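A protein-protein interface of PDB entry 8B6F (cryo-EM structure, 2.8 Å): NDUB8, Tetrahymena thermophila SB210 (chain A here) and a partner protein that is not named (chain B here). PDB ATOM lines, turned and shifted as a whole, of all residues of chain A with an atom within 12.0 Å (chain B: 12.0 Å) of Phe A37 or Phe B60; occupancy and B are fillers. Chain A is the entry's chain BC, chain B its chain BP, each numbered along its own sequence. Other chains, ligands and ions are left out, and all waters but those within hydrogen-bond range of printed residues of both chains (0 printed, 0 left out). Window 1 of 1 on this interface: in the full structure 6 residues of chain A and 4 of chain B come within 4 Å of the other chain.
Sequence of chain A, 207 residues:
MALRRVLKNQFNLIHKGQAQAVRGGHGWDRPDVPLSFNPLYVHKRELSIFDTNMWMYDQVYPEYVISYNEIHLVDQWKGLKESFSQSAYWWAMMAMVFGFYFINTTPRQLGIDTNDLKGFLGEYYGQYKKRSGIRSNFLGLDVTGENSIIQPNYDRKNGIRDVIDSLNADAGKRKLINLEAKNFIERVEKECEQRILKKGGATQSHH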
ATOM      1  N   ARG A  30     -23.709  -4.072 -37.799  1.00  0.00           N
ATOM      2  CA  ARG A  30     -23.707  -2.893 -36.956  1.00  0.00           C
ATOM      3  C   ARG A  30     -22.319  -2.600 -36.383  1.00  0.00           C
ATOM      4  O   ARG A  30     -21.579  -3.527 -36.044  1.00  0.00           O
ATOM      5  CB  ARG A  30     -24.725  -3.082 -35.839  1.00  0.00           C
ATOM      6  CG  ARG A  30     -26.149  -3.117 -36.374  1.00  0.00           C
ATOM      7  CD  ARG A  30     -27.151  -3.583 -35.340  1.00  0.00           C
ATOM      8  NE  ARG A  30     -26.999  -2.883 -34.073  1.00  0.00           N
ATOM      9  CZ  ARG A  30     -27.417  -1.645 -33.851  1.00  0.00           C
ATOM     10  NH1 ARG A  30     -28.022  -0.940 -34.792  1.00  0.00           N
ATOM     11  NH2 ARG A  30     -27.226  -1.102 -32.655  1.00  0.00           N
ATOM     12  N   PRO A  31     -21.942  -1.332 -36.257  1.00  0.00           N
ATOM     13  CA  PRO A  31     -20.672  -0.988 -35.607  1.00  0.00           C
ATOM     14  C   PRO A  31     -20.751  -1.299 -34.114  1.00  0.00           C
ATOM     15  O   PRO A  31     -21.834  -1.383 -33.534  1.00  0.00           O
ATOM     16  CB  PRO A  31     -20.490   0.507 -35.903  1.00  0.00           C
ATOM     17  CG  PRO A  31     -21.821   1.006 -36.207  1.00  0.00           C
ATOM     18  CD  PRO A  31     -22.596  -0.138 -36.810  1.00  0.00           C
ATOM     19  N   ASP A  32     -19.590  -1.474 -33.482  1.00  0.00           N
ATOM     20  CA  ASP A  32     -19.562  -1.913 -32.089  1.00  0.00           C
ATOM     21  C   ASP A  32     -20.237  -0.866 -31.208  1.00  0.00           C
ATOM     22  O   ASP A  32     -20.244   0.325 -31.529  1.00  0.00           O
ATOM     23  CB  ASP A  32     -18.128  -2.133 -31.610  1.00  0.00           C
ATOM     24  CG  ASP A  32     -17.712  -3.588 -31.654  1.00  0.00           C
ATOM     25  OD1 ASP A  32     -18.295  -4.351 -32.452  1.00  0.00           O
ATOM     26  OD2 ASP A  32     -16.806  -3.971 -30.885  1.00  0.00           O
ATOM     27  N   VAL A  33     -20.821  -1.311 -30.095  1.00  0.00           N
ATOM     28  CA  VAL A  33     -21.729  -0.452 -29.336  1.00  0.00           C
ATOM     29  C   VAL A  33     -21.028   0.865 -29.027  1.00  0.00           C
ATOM     30  O   VAL A  33     -19.860   0.876 -28.613  1.00  0.00           O
ATOM     31  CB  VAL A  33     -22.168  -1.142 -28.030  1.00  0.00           C
ATOM     32  CG1 VAL A  33     -22.874  -0.172 -27.080  1.00  0.00           C
ATOM     33  CG2 VAL A  33     -23.055  -2.342 -28.319  1.00  0.00           C
ATOM     34  N   PRO A  34     -21.709   1.993 -29.218  1.00  0.00           N
ATOM     35  CA  PRO A  34     -21.054   3.295 -29.061  1.00  0.00           C
ATOM     36  C   PRO A  34     -20.635   3.641 -27.643  1.00  0.00           C
ATOM     37  O   PRO A  34     -21.332   3.335 -26.673  1.00  0.00           O
ATOM     38  CB  PRO A  34     -22.120   4.277 -29.561  1.00  0.00           C
ATOM     39  CG  PRO A  34     -23.395   3.590 -29.286  1.00  0.00           C
ATOM     40  CD  PRO A  34     -23.128   2.151 -29.587  1.00  0.00           C
ATOM     41  N   LEU A  35     -19.476   4.291 -27.535  1.00  0.00           N
ATOM     42  CA  LEU A  35     -19.001   4.781 -26.248  1.00  0.00           C
ATOM     43  C   LEU A  35     -19.911   5.917 -25.791  1.00  0.00           C
ATOM     44  O   LEU A  35     -19.944   6.256 -24.604  1.00  0.00           O
ATOM     45  CB  LEU A  35     -17.533   5.193 -26.324  1.00  0.00           C
ATOM     46  CG  LEU A  35     -16.615   3.972 -26.189  1.00  0.00           C
ATOM     47  CD1 LEU A  35     -15.284   4.187 -26.880  1.00  0.00           C
ATOM     48  CD2 LEU A  35     -16.399   3.614 -24.724  1.00  0.00           C
ATOM     49  N   SER A  36     -20.643   6.493 -26.752  1.00  0.00           N
ATOM     50  CA  SER A  36     -21.618   7.563 -26.561  1.00  0.00           C
ATOM     51  C   SER A  36     -22.785   7.093 -25.708  1.00  0.00           C
ATOM     52  O   SER A  36     -23.505   7.925 -25.146  1.00  0.00           O
ATOM     53  CB  SER A  36     -22.118   8.082 -27.909  1.00  0.00           C
ATOM     54  OG  SER A  36     -23.386   7.540 -28.233  1.00  0.00           O
ATOM     55  N   PHE A  37     -22.991   5.779 -25.613  1.00  0.00           N
ATOM     56  CA  PHE A  37     -24.104   5.251 -24.835  1.00  0.00           C
ATOM     57  C   PHE A  37     -23.952   5.731 -23.399  1.00  0.00           C
ATOM     58  O   PHE A  37     -24.939   6.101 -22.754  1.00  0.00           O
ATOM     59  CB  PHE A  37     -24.106   3.722 -24.954  1.00  0.00           C
ATOM     60  CG  PHE A  37     -25.108   3.013 -24.081  1.00  0.00           C
ATOM     61  CD1 PHE A  37     -24.860   2.805 -22.734  1.00  0.00           C
ATOM     62  CD2 PHE A  37     -26.276   2.507 -24.626  1.00  0.00           C
ATOM     63  CE1 PHE A  37     -25.772   2.131 -21.942  1.00  0.00           C
ATOM     64  CE2 PHE A  37     -27.193   1.837 -23.839  1.00  0.00           C
ATOM     65  CZ  PHE A  37     -26.939   1.647 -22.496  1.00  0.00           C
ATOM     66  N   ASN A  38     -22.725   5.733 -22.880  1.00  0.00           N
ATOM     67  CA  ASN A  38     -22.487   6.378 -21.599  1.00  0.00           C
ATOM     68  C   ASN A  38     -21.819   7.702 -21.953  1.00  0.00           C
ATOM     69  O   ASN A  38     -20.648   7.706 -22.359  1.00  0.00           O
ATOM     70  CB  ASN A  38     -21.590   5.533 -20.701  1.00  0.00           C
ATOM     71  CG  ASN A  38     -22.106   4.122 -20.545  1.00  0.00           C
ATOM     72  OD1 ASN A  38     -21.409   3.156 -20.850  1.00  0.00           O
ATOM     73  ND2 ASN A  38     -23.351   3.996 -20.099  1.00  0.00           N
ATOM     74  N   PRO A  39     -22.519   8.843 -21.816  1.00  0.00           N
ATOM     75  CA  PRO A  39     -21.910  10.162 -22.070  1.00  0.00           C
ATOM     76  C   PRO A  39     -21.192  10.815 -20.904  1.00  0.00           C
ATOM     77  O   PRO A  39     -21.793  10.984 -19.840  1.00  0.00           O
ATOM     78  CB  PRO A  39     -23.122  11.009 -22.474  1.00  0.00           C
ATOM     79  CG  PRO A  39     -24.225  10.424 -21.678  1.00  0.00           C
ATOM     80  CD  PRO A  39     -23.983   8.943 -21.691  1.00  0.00           C
ATOM     81  N   LEU A  40     -19.925  11.190 -21.066  1.00  0.00           N
ATOM     82  CA  LEU A  40     -19.213  11.788 -19.947  1.00  0.00           C
ATOM     83  C   LEU A  40     -19.902  13.084 -19.545  1.00  0.00           C
ATOM     84  O   LEU A  40     -20.249  13.909 -20.393  1.00  0.00           O
ATOM     85  CB  LEU A  40     -17.758  12.067 -20.329  1.00  0.00           C
ATOM     86  CG  LEU A  40     -16.888  12.687 -19.232  1.00  0.00           C
ATOM     87  CD1 LEU A  40     -16.765  11.762 -18.036  1.00  0.00           C
ATOM     88  CD2 LEU A  40     -15.515  13.052 -19.773  1.00  0.00           C
ATOM     89  N   TYR A  41     -20.088  13.263 -18.241  1.00  0.00           N
ATOM     90  CA  TYR A  41     -20.734  14.443 -17.683  1.00  0.00           C
ATOM     91  C   TYR A  41     -19.673  15.459 -17.277  1.00  0.00           C
ATOM     92  O   TYR A  41     -18.782  15.141 -16.483  1.00  0.00           O
ATOM     93  CB  TYR A  41     -21.609  14.062 -16.490  1.00  0.00           C
ATOM     94  CG  TYR A  41     -22.232  15.245 -15.792  1.00  0.00           C
ATOM     95  CD1 TYR A  41     -23.423  15.791 -16.248  1.00  0.00           C
ATOM     96  CD2 TYR A  41     -21.636  15.813 -14.678  1.00  0.00           C
ATOM     97  CE1 TYR A  41     -23.999  16.871 -15.617  1.00  0.00           C
ATOM     98  CE2 TYR A  41     -22.205  16.895 -14.039  1.00  0.00           C
ATOM     99  CZ  TYR A  41     -23.387  17.418 -14.513  1.00  0.00           C
ATOM    100  OH  TYR A  41     -23.960  18.495 -13.882  1.00  0.00           O
ATOM    101  N   ASP A  58     -22.592  11.224  -9.962  1.00  0.00           N
ATOM    102  CA  ASP A  58     -22.252  10.257 -10.992  1.00  0.00           C
ATOM    103  C   ASP A  58     -21.416  10.956 -12.052  1.00  0.00           C
ATOM    104  O   ASP A  58     -21.440  12.182 -12.179  1.00  0.00           O
ATOM    105  CB  ASP A  58     -23.505   9.637 -11.619  1.00  0.00           C
ATOM    106  CG  ASP A  58     -23.186   8.455 -12.507  1.00  0.00           C
ATOM    107  OD1 ASP A  58     -22.005   8.059 -12.564  1.00  0.00           O
ATOM    108  OD2 ASP A  58     -24.113   7.920 -13.148  1.00  0.00           O
ATOM    109  N   GLN A  59     -20.668  10.160 -12.808  1.00  0.00           N
ATOM    110  CA  GLN A  59     -19.818  10.678 -13.870  1.00  0.00           C
ATOM    111  C   GLN A  59     -20.491  10.652 -15.235  1.00  0.00           C
ATOM    112  O   GLN A  59     -19.893  11.119 -16.209  1.00  0.00           O
ATOM    113  CB  GLN A  59     -18.511   9.882 -13.926  1.00  0.00           C
ATOM    114  CG  GLN A  59     -17.733   9.908 -12.623  1.00  0.00           C
ATOM    115  CD  GLN A  59     -16.444   9.126 -12.700  1.00  0.00           C
ATOM    116  OE1 GLN A  59     -16.042   8.675 -13.770  1.00  0.00           O
ATOM    117  NE2 GLN A  59     -15.787   8.957 -11.560  1.00  0.00           N
ATOM    118  N   VAL A  60     -21.708  10.122 -15.332  1.00  0.00           N
ATOM    119  CA  VAL A  60     -22.414  10.045 -16.605  1.00  0.00           C
ATOM    120  C   VAL A  60     -23.774  10.717 -16.476  1.00  0.00           C
ATOM    121  O   VAL A  60     -24.095  11.645 -17.226  1.00  0.00           O
ATOM    122  CB  VAL A  60     -22.560   8.582 -17.065  1.00  0.00           C
ATOM    123  CG1 VAL A  60     -23.345   8.498 -18.362  1.00  0.00           C
ATOM    124  CG2 VAL A  60     -21.195   7.945 -17.231  1.00  0.00           C
ATOM    125  N   TYR A  61     -24.582  10.255 -15.524  1.00  0.00           N
ATOM    126  CA  TYR A  61     -25.946  10.747 -15.324  1.00  0.00           C
ATOM    127  C   TYR A  61     -26.155  11.076 -13.852  1.00  0.00           C
ATOM    128  O   TYR A  61     -26.850  10.350 -13.133  1.00  0.00           O
ATOM    129  CB  TYR A  61     -26.971   9.716 -15.797  1.00  0.00           C
ATOM    130  CG  TYR A  61     -27.001   9.496 -17.293  1.00  0.00           C
ATOM    131  CD1 TYR A  61     -26.865  10.558 -18.178  1.00  0.00           C
ATOM    132  CD2 TYR A  61     -27.169   8.223 -17.819  1.00  0.00           C
ATOM    133  CE1 TYR A  61     -26.895  10.359 -19.542  1.00  0.00           C
ATOM    134  CE2 TYR A  61     -27.199   8.013 -19.181  1.00  0.00           C
ATOM    135  CZ  TYR A  61     -27.061   9.084 -20.038  1.00  0.00           C
ATOM    136  OH  TYR A  61     -27.092   8.874 -21.397  1.00  0.00           O
ATOM    137  N   PRO A  62     -25.566  12.168 -13.370  1.00  0.00           N
ATOM    138  CA  PRO A  62     -25.840  12.590 -11.992  1.00  0.00           C
ATOM    139  C   PRO A  62     -27.306  12.950 -11.815  1.00  0.00           C
ATOM    140  O   PRO A  62     -27.961  13.451 -12.731  1.00  0.00           O
ATOM    141  CB  PRO A  62     -24.930  13.811 -11.805  1.00  0.00           C
ATOM    142  CG  PRO A  62     -24.672  14.306 -13.178  1.00  0.00           C
ATOM    143  CD  PRO A  62     -24.664  13.100 -14.065  1.00  0.00           C
ATOM    144  N   GLU A  63     -27.821  12.688 -10.617  1.00  0.00           N
ATOM    145  CA  GLU A  63     -29.233  12.879 -10.332  1.00  0.00           C
ATOM    146  C   GLU A  63     -29.406  13.466  -8.940  1.00  0.00           C
ATOM    147  O   GLU A  63     -28.568  13.268  -8.058  1.00  0.00           O
ATOM    148  CB  GLU A  63     -30.005  11.559 -10.430  1.00  0.00           C
ATOM    149  CG  GLU A  63     -29.922  10.906 -11.798  1.00  0.00           C
ATOM    150  CD  GLU A  63     -30.792   9.673 -11.906  1.00  0.00           C
ATOM    151  OE1 GLU A  63     -31.653   9.475 -11.025  1.00  0.00           O
ATOM    152  OE2 GLU A  63     -30.613   8.900 -12.870  1.00  0.00           O
ATOM    153  N   GLY B  58     -33.754  -8.888 -28.291  1.00  0.00           N
ATOM    154  CA  GLY B  58     -34.217  -8.988 -26.879  1.00  0.00           C
ATOM    155  C   GLY B  58     -33.251  -8.349 -25.903  1.00  0.00           C
ATOM    156  O   GLY B  58     -33.551  -7.316 -25.304  1.00  0.00           O
ATOM    157  N   GLY B  59     -32.086  -8.970 -25.735  1.00  0.00           N
ATOM    158  CA  GLY B  59     -31.061  -8.435 -24.869  1.00  0.00           C
ATOM    159  C   GLY B  59     -30.260  -7.340 -25.544  1.00  0.00           C
ATOM    160  O   GLY B  59     -30.425  -7.030 -26.723  1.00  0.00           O
ATOM    161  N   PHE B  60     -29.368  -6.740 -24.764  1.00  0.00           N
ATOM    162  CA  PHE B  60     -28.522  -5.674 -25.277  1.00  0.00           C
ATOM    163  C   PHE B  60     -27.461  -6.241 -26.215  1.00  0.00           C
ATOM    164  O   PHE B  60     -27.082  -7.411 -26.128  1.00  0.00           O
ATOM    165  CB  PHE B  60     -27.861  -4.924 -24.122  1.00  0.00           C
ATOM    166  CG  PHE B  60     -27.181  -3.655 -24.535  1.00  0.00           C
ATOM    167  CD1 PHE B  60     -27.922  -2.528 -24.839  1.00  0.00           C
ATOM    168  CD2 PHE B  60     -25.801  -3.583 -24.599  1.00  0.00           C
ATOM    169  CE1 PHE B  60     -27.301  -1.355 -25.212  1.00  0.00           C
ATOM    170  CE2 PHE B  60     -25.172  -2.413 -24.971  1.00  0.00           C
ATOM    171  CZ  PHE B  60     -25.924  -1.296 -25.278  1.00  0.00           C
ATOM    172  N   GLN B  61     -26.990  -5.395 -27.127  1.00  0.00           N
ATOM    173  CA  GLN B  61     -25.956  -5.809 -28.063  1.00  0.00           C
ATOM    174  C   GLN B  61     -24.652  -6.084 -27.327  1.00  0.00           C
ATOM    175  O   GLN B  61     -24.265  -5.348 -26.416  1.00  0.00           O
ATOM    176  CB  GLN B  61     -25.738  -4.734 -29.127  1.00  0.00           C
ATOM    177  CG  GLN B  61     -24.661  -5.080 -30.144  1.00  0.00           C
ATOM    178  CD  GLN B  61     -24.508  -4.016 -31.207  1.00  0.00           C
ATOM    179  OE1 GLN B  61     -25.378  -3.165 -31.377  1.00  0.00           O
ATOM    180  NE2 GLN B  61     -23.394  -4.054 -31.927  1.00  0.00           N
ATOM    181  N   LYS B  62     -23.969  -7.151 -27.730  1.00  0.00           N
ATOM    182  CA  LYS B  62     -22.724  -7.526 -27.078  1.00  0.00           C
ATOM    183  C   LYS B  62     -21.603  -6.571 -27.466  1.00  0.00           C
ATOM    184  O   LYS B  62     -21.489  -6.156 -28.622  1.00  0.00           O
ATOM    185  CB  LYS B  62     -22.353  -8.962 -27.442  1.00  0.00           C
ATOM    186  CG  LYS B  62     -23.444  -9.960 -27.092  1.00  0.00           C
ATOM    187  CD  LYS B  62     -23.013 -11.399 -27.301  1.00  0.00           C
ATOM    188  CE  LYS B  62     -24.139 -12.342 -26.909  1.00  0.00           C
ATOM    189  NZ  LYS B  62     -23.786 -13.770 -27.099  1.00  0.00           N
ATOM    190  N   TYR B  63     -20.778  -6.219 -26.488  1.00  0.00           N
ATOM    191  CA  TYR B  63     -19.659  -5.314 -26.673  1.00  0.00           C
ATOM    192  C   TYR B  63     -18.402  -5.918 -26.064  1.00  0.00           C
ATOM    193  O   TYR B  63     -18.486  -6.743 -25.150  1.00  0.00           O
ATOM    194  CB  TYR B  63     -19.941  -3.948 -26.030  1.00  0.00           C
ATOM    195  CG  TYR B  63     -20.445  -4.036 -24.610  1.00  0.00           C
ATOM    196  CD1 TYR B  63     -19.561  -4.091 -23.543  1.00  0.00           C
ATOM    197  CD2 TYR B  63     -21.805  -4.057 -24.337  1.00  0.00           C
ATOM    198  CE1 TYR B  63     -20.017  -4.169 -22.242  1.00  0.00           C
ATOM    199  CE2 TYR B  63     -22.271  -4.137 -23.041  1.00  0.00           C
ATOM    200  CZ  TYR B  63     -21.372  -4.192 -21.998  1.00  0.00           C
ATOM    201  OH  TYR B  63     -21.830  -4.270 -20.704  1.00  0.00           O
ATOM    202  N   PRO B  64     -17.225  -5.532 -26.555  1.00  0.00           N
ATOM    203  CA  PRO B  64     -15.986  -6.134 -26.047  1.00  0.00           C
ATOM    204  C   PRO B  64     -15.764  -5.843 -24.570  1.00  0.00           C
ATOM    205  O   PRO B  64     -16.099  -4.771 -24.065  1.00  0.00           O
ATOM    206  CB  PRO B  64     -14.896  -5.490 -26.914  1.00  0.00           C
ATOM    207  CG  PRO B  64     -15.505  -4.240 -27.430  1.00  0.00           C
ATOM    208  CD  PRO B  64     -16.959  -4.534 -27.605  1.00  0.00           C
ATOM    209  N   ILE B  65     -15.180  -6.820 -23.883  1.00  0.00           N
ATOM    210  CA  ILE B  65     -14.838  -6.717 -22.471  1.00  0.00           C
ATOM    211  C   ILE B  65     -13.327  -6.864 -22.360  1.00  0.00           C
ATOM    212  O   ILE B  65     -12.762  -7.776 -22.965  1.00  0.00           O
ATOM    213  CB  ILE B  65     -15.540  -7.789 -21.617  1.00  0.00           C
ATOM    214  CG1 ILE B  65     -17.057  -7.747 -21.832  1.00  0.00           C
ATOM    215  CG2 ILE B  65     -15.195  -7.615 -20.144  1.00  0.00           C
ATOM    216  CD1 ILE B  65     -17.718  -6.452 -21.410  1.00  0.00           C
ATOM    217  N   GLN B  73     -19.226 -10.556 -17.505  1.00  0.00           N
ATOM    218  CA  GLN B  73     -20.009 -10.217 -18.687  1.00  0.00           C
ATOM    219  C   GLN B  73     -19.894 -11.299 -19.752  1.00  0.00           C
ATOM    220  O   GLN B  73     -18.828 -11.482 -20.347  1.00  0.00           O
ATOM    221  CB  GLN B  73     -19.565  -8.871 -19.265  1.00  0.00           C
ATOM    222  CG  GLN B  73     -20.066  -7.652 -18.504  1.00  0.00           C
ATOM    223  CD  GLN B  73     -19.473  -7.540 -17.119  1.00  0.00           C
ATOM    224  OE1 GLN B  73     -19.151  -8.544 -16.486  1.00  0.00           O
ATOM    225  NE2 GLN B  73     -19.317  -6.313 -16.639  1.00  0.00           N
ATOM    226  N   TRP B  74     -20.991 -12.010 -20.007  1.00  0.00           N
ATOM    227  CA  TRP B  74     -21.052 -13.023 -21.060  1.00  0.00           C
ATOM    228  C   TRP B  74     -19.944 -14.063 -20.904  1.00  0.00           C
ATOM    229  O   TRP B  74     -19.243 -14.407 -21.858  1.00  0.00           O
ATOM    230  CB  TRP B  74     -20.989 -12.374 -22.442  1.00  0.00           C
ATOM    231  CG  TRP B  74     -22.226 -11.626 -22.820  1.00  0.00           C
ATOM    232  CD1 TRP B  74     -23.453 -12.157 -23.080  1.00  0.00           C
ATOM    233  CD2 TRP B  74     -22.353 -10.211 -22.995  1.00  0.00           C
ATOM    234  NE1 TRP B  74     -24.339 -11.161 -23.402  1.00  0.00           N
ATOM    235  CE2 TRP B  74     -23.691  -9.956 -23.355  1.00  0.00           C
ATOM    236  CE3 TRP B  74     -21.469  -9.136 -22.877  1.00  0.00           C
ATOM    237  CZ2 TRP B  74     -24.164  -8.670 -23.602  1.00  0.00           C
ATOM    238  CZ3 TRP B  74     -21.941  -7.859 -23.121  1.00  0.00           C
ATOM    239  CH2 TRP B  74     -23.276  -7.636 -23.479  1.00  0.00           C
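NH2 of Arg A30 sits at hydrogen-bond distance from OE1 of Gln B61 (3.1 Å). NE2 of Gln B61 sits at hydrogen-bond distance from O of Pro A31 (3.5 Å).
Among the printed residues, merely in contact across the chains: Asp A32 with Pro B64 (3.3 Å), Val A33 with Phe B60 (3.7 Å), Val A33 with Gln B61 (3.6 Å) and Phe A37 with Phe B60 (3.5 Å).
Of the printed residues of chain B, Pro A31 touches Gln B61 (3.5 Å). Printed residues of chain B within 4 Å of Asp A32: Pro B64. Of chain B, only Phe B60 and Gln B61 come within 4 Å of Val A33. No residue of chain B comes within 4 Å of Pro A34. Ser A36 touches none of the printed residues of chain B. Phe A37 touches just one residue of chain B: Phe B60 (3.5 Å). Gly B58 touches none of the printed residues of chain A. No residue of chain A comes within 4 Å of Gly B59. Phe B60 touches two residues of chain A. Of chain A, only Arg A30 (3.1 Å), Pro A31 (3.5 Å) and Val A33 (3.6 Å) come within 4 Å of Gln B61. Printed residues of chain A within 4 Å of Pro B64: Asp A32. The nearest residue of chain A that does not touch Phe B60 is Pro A34 (6.2 Å). The nearest printed residue of chain B that does not touch Arg A30 is Phe B60 (7.4 Å).
Of the 10 printed residues of chain B, 3 touch a printed residue of chain A. Printed residues of chain B that touch a printed residue of chain A: Phe B60, Gln B61 and Pro B64. Hydrophobic or aromatic side chains of chain B within 4 Å of the printed part of chain A: Phe B60 and Pro B64. Of the 18 printed residues of chain A, 5 touch a printed residue of chain B. Hydrophobic or aromatic side chains of chain A within 4 Å of the printed part of chain B: Val A33 and Phe A37. Among the printed residues, no Asp or Glu carboxylate lies within 4 Å of a Lys or Arg side-chain nitrogen of the other chain.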
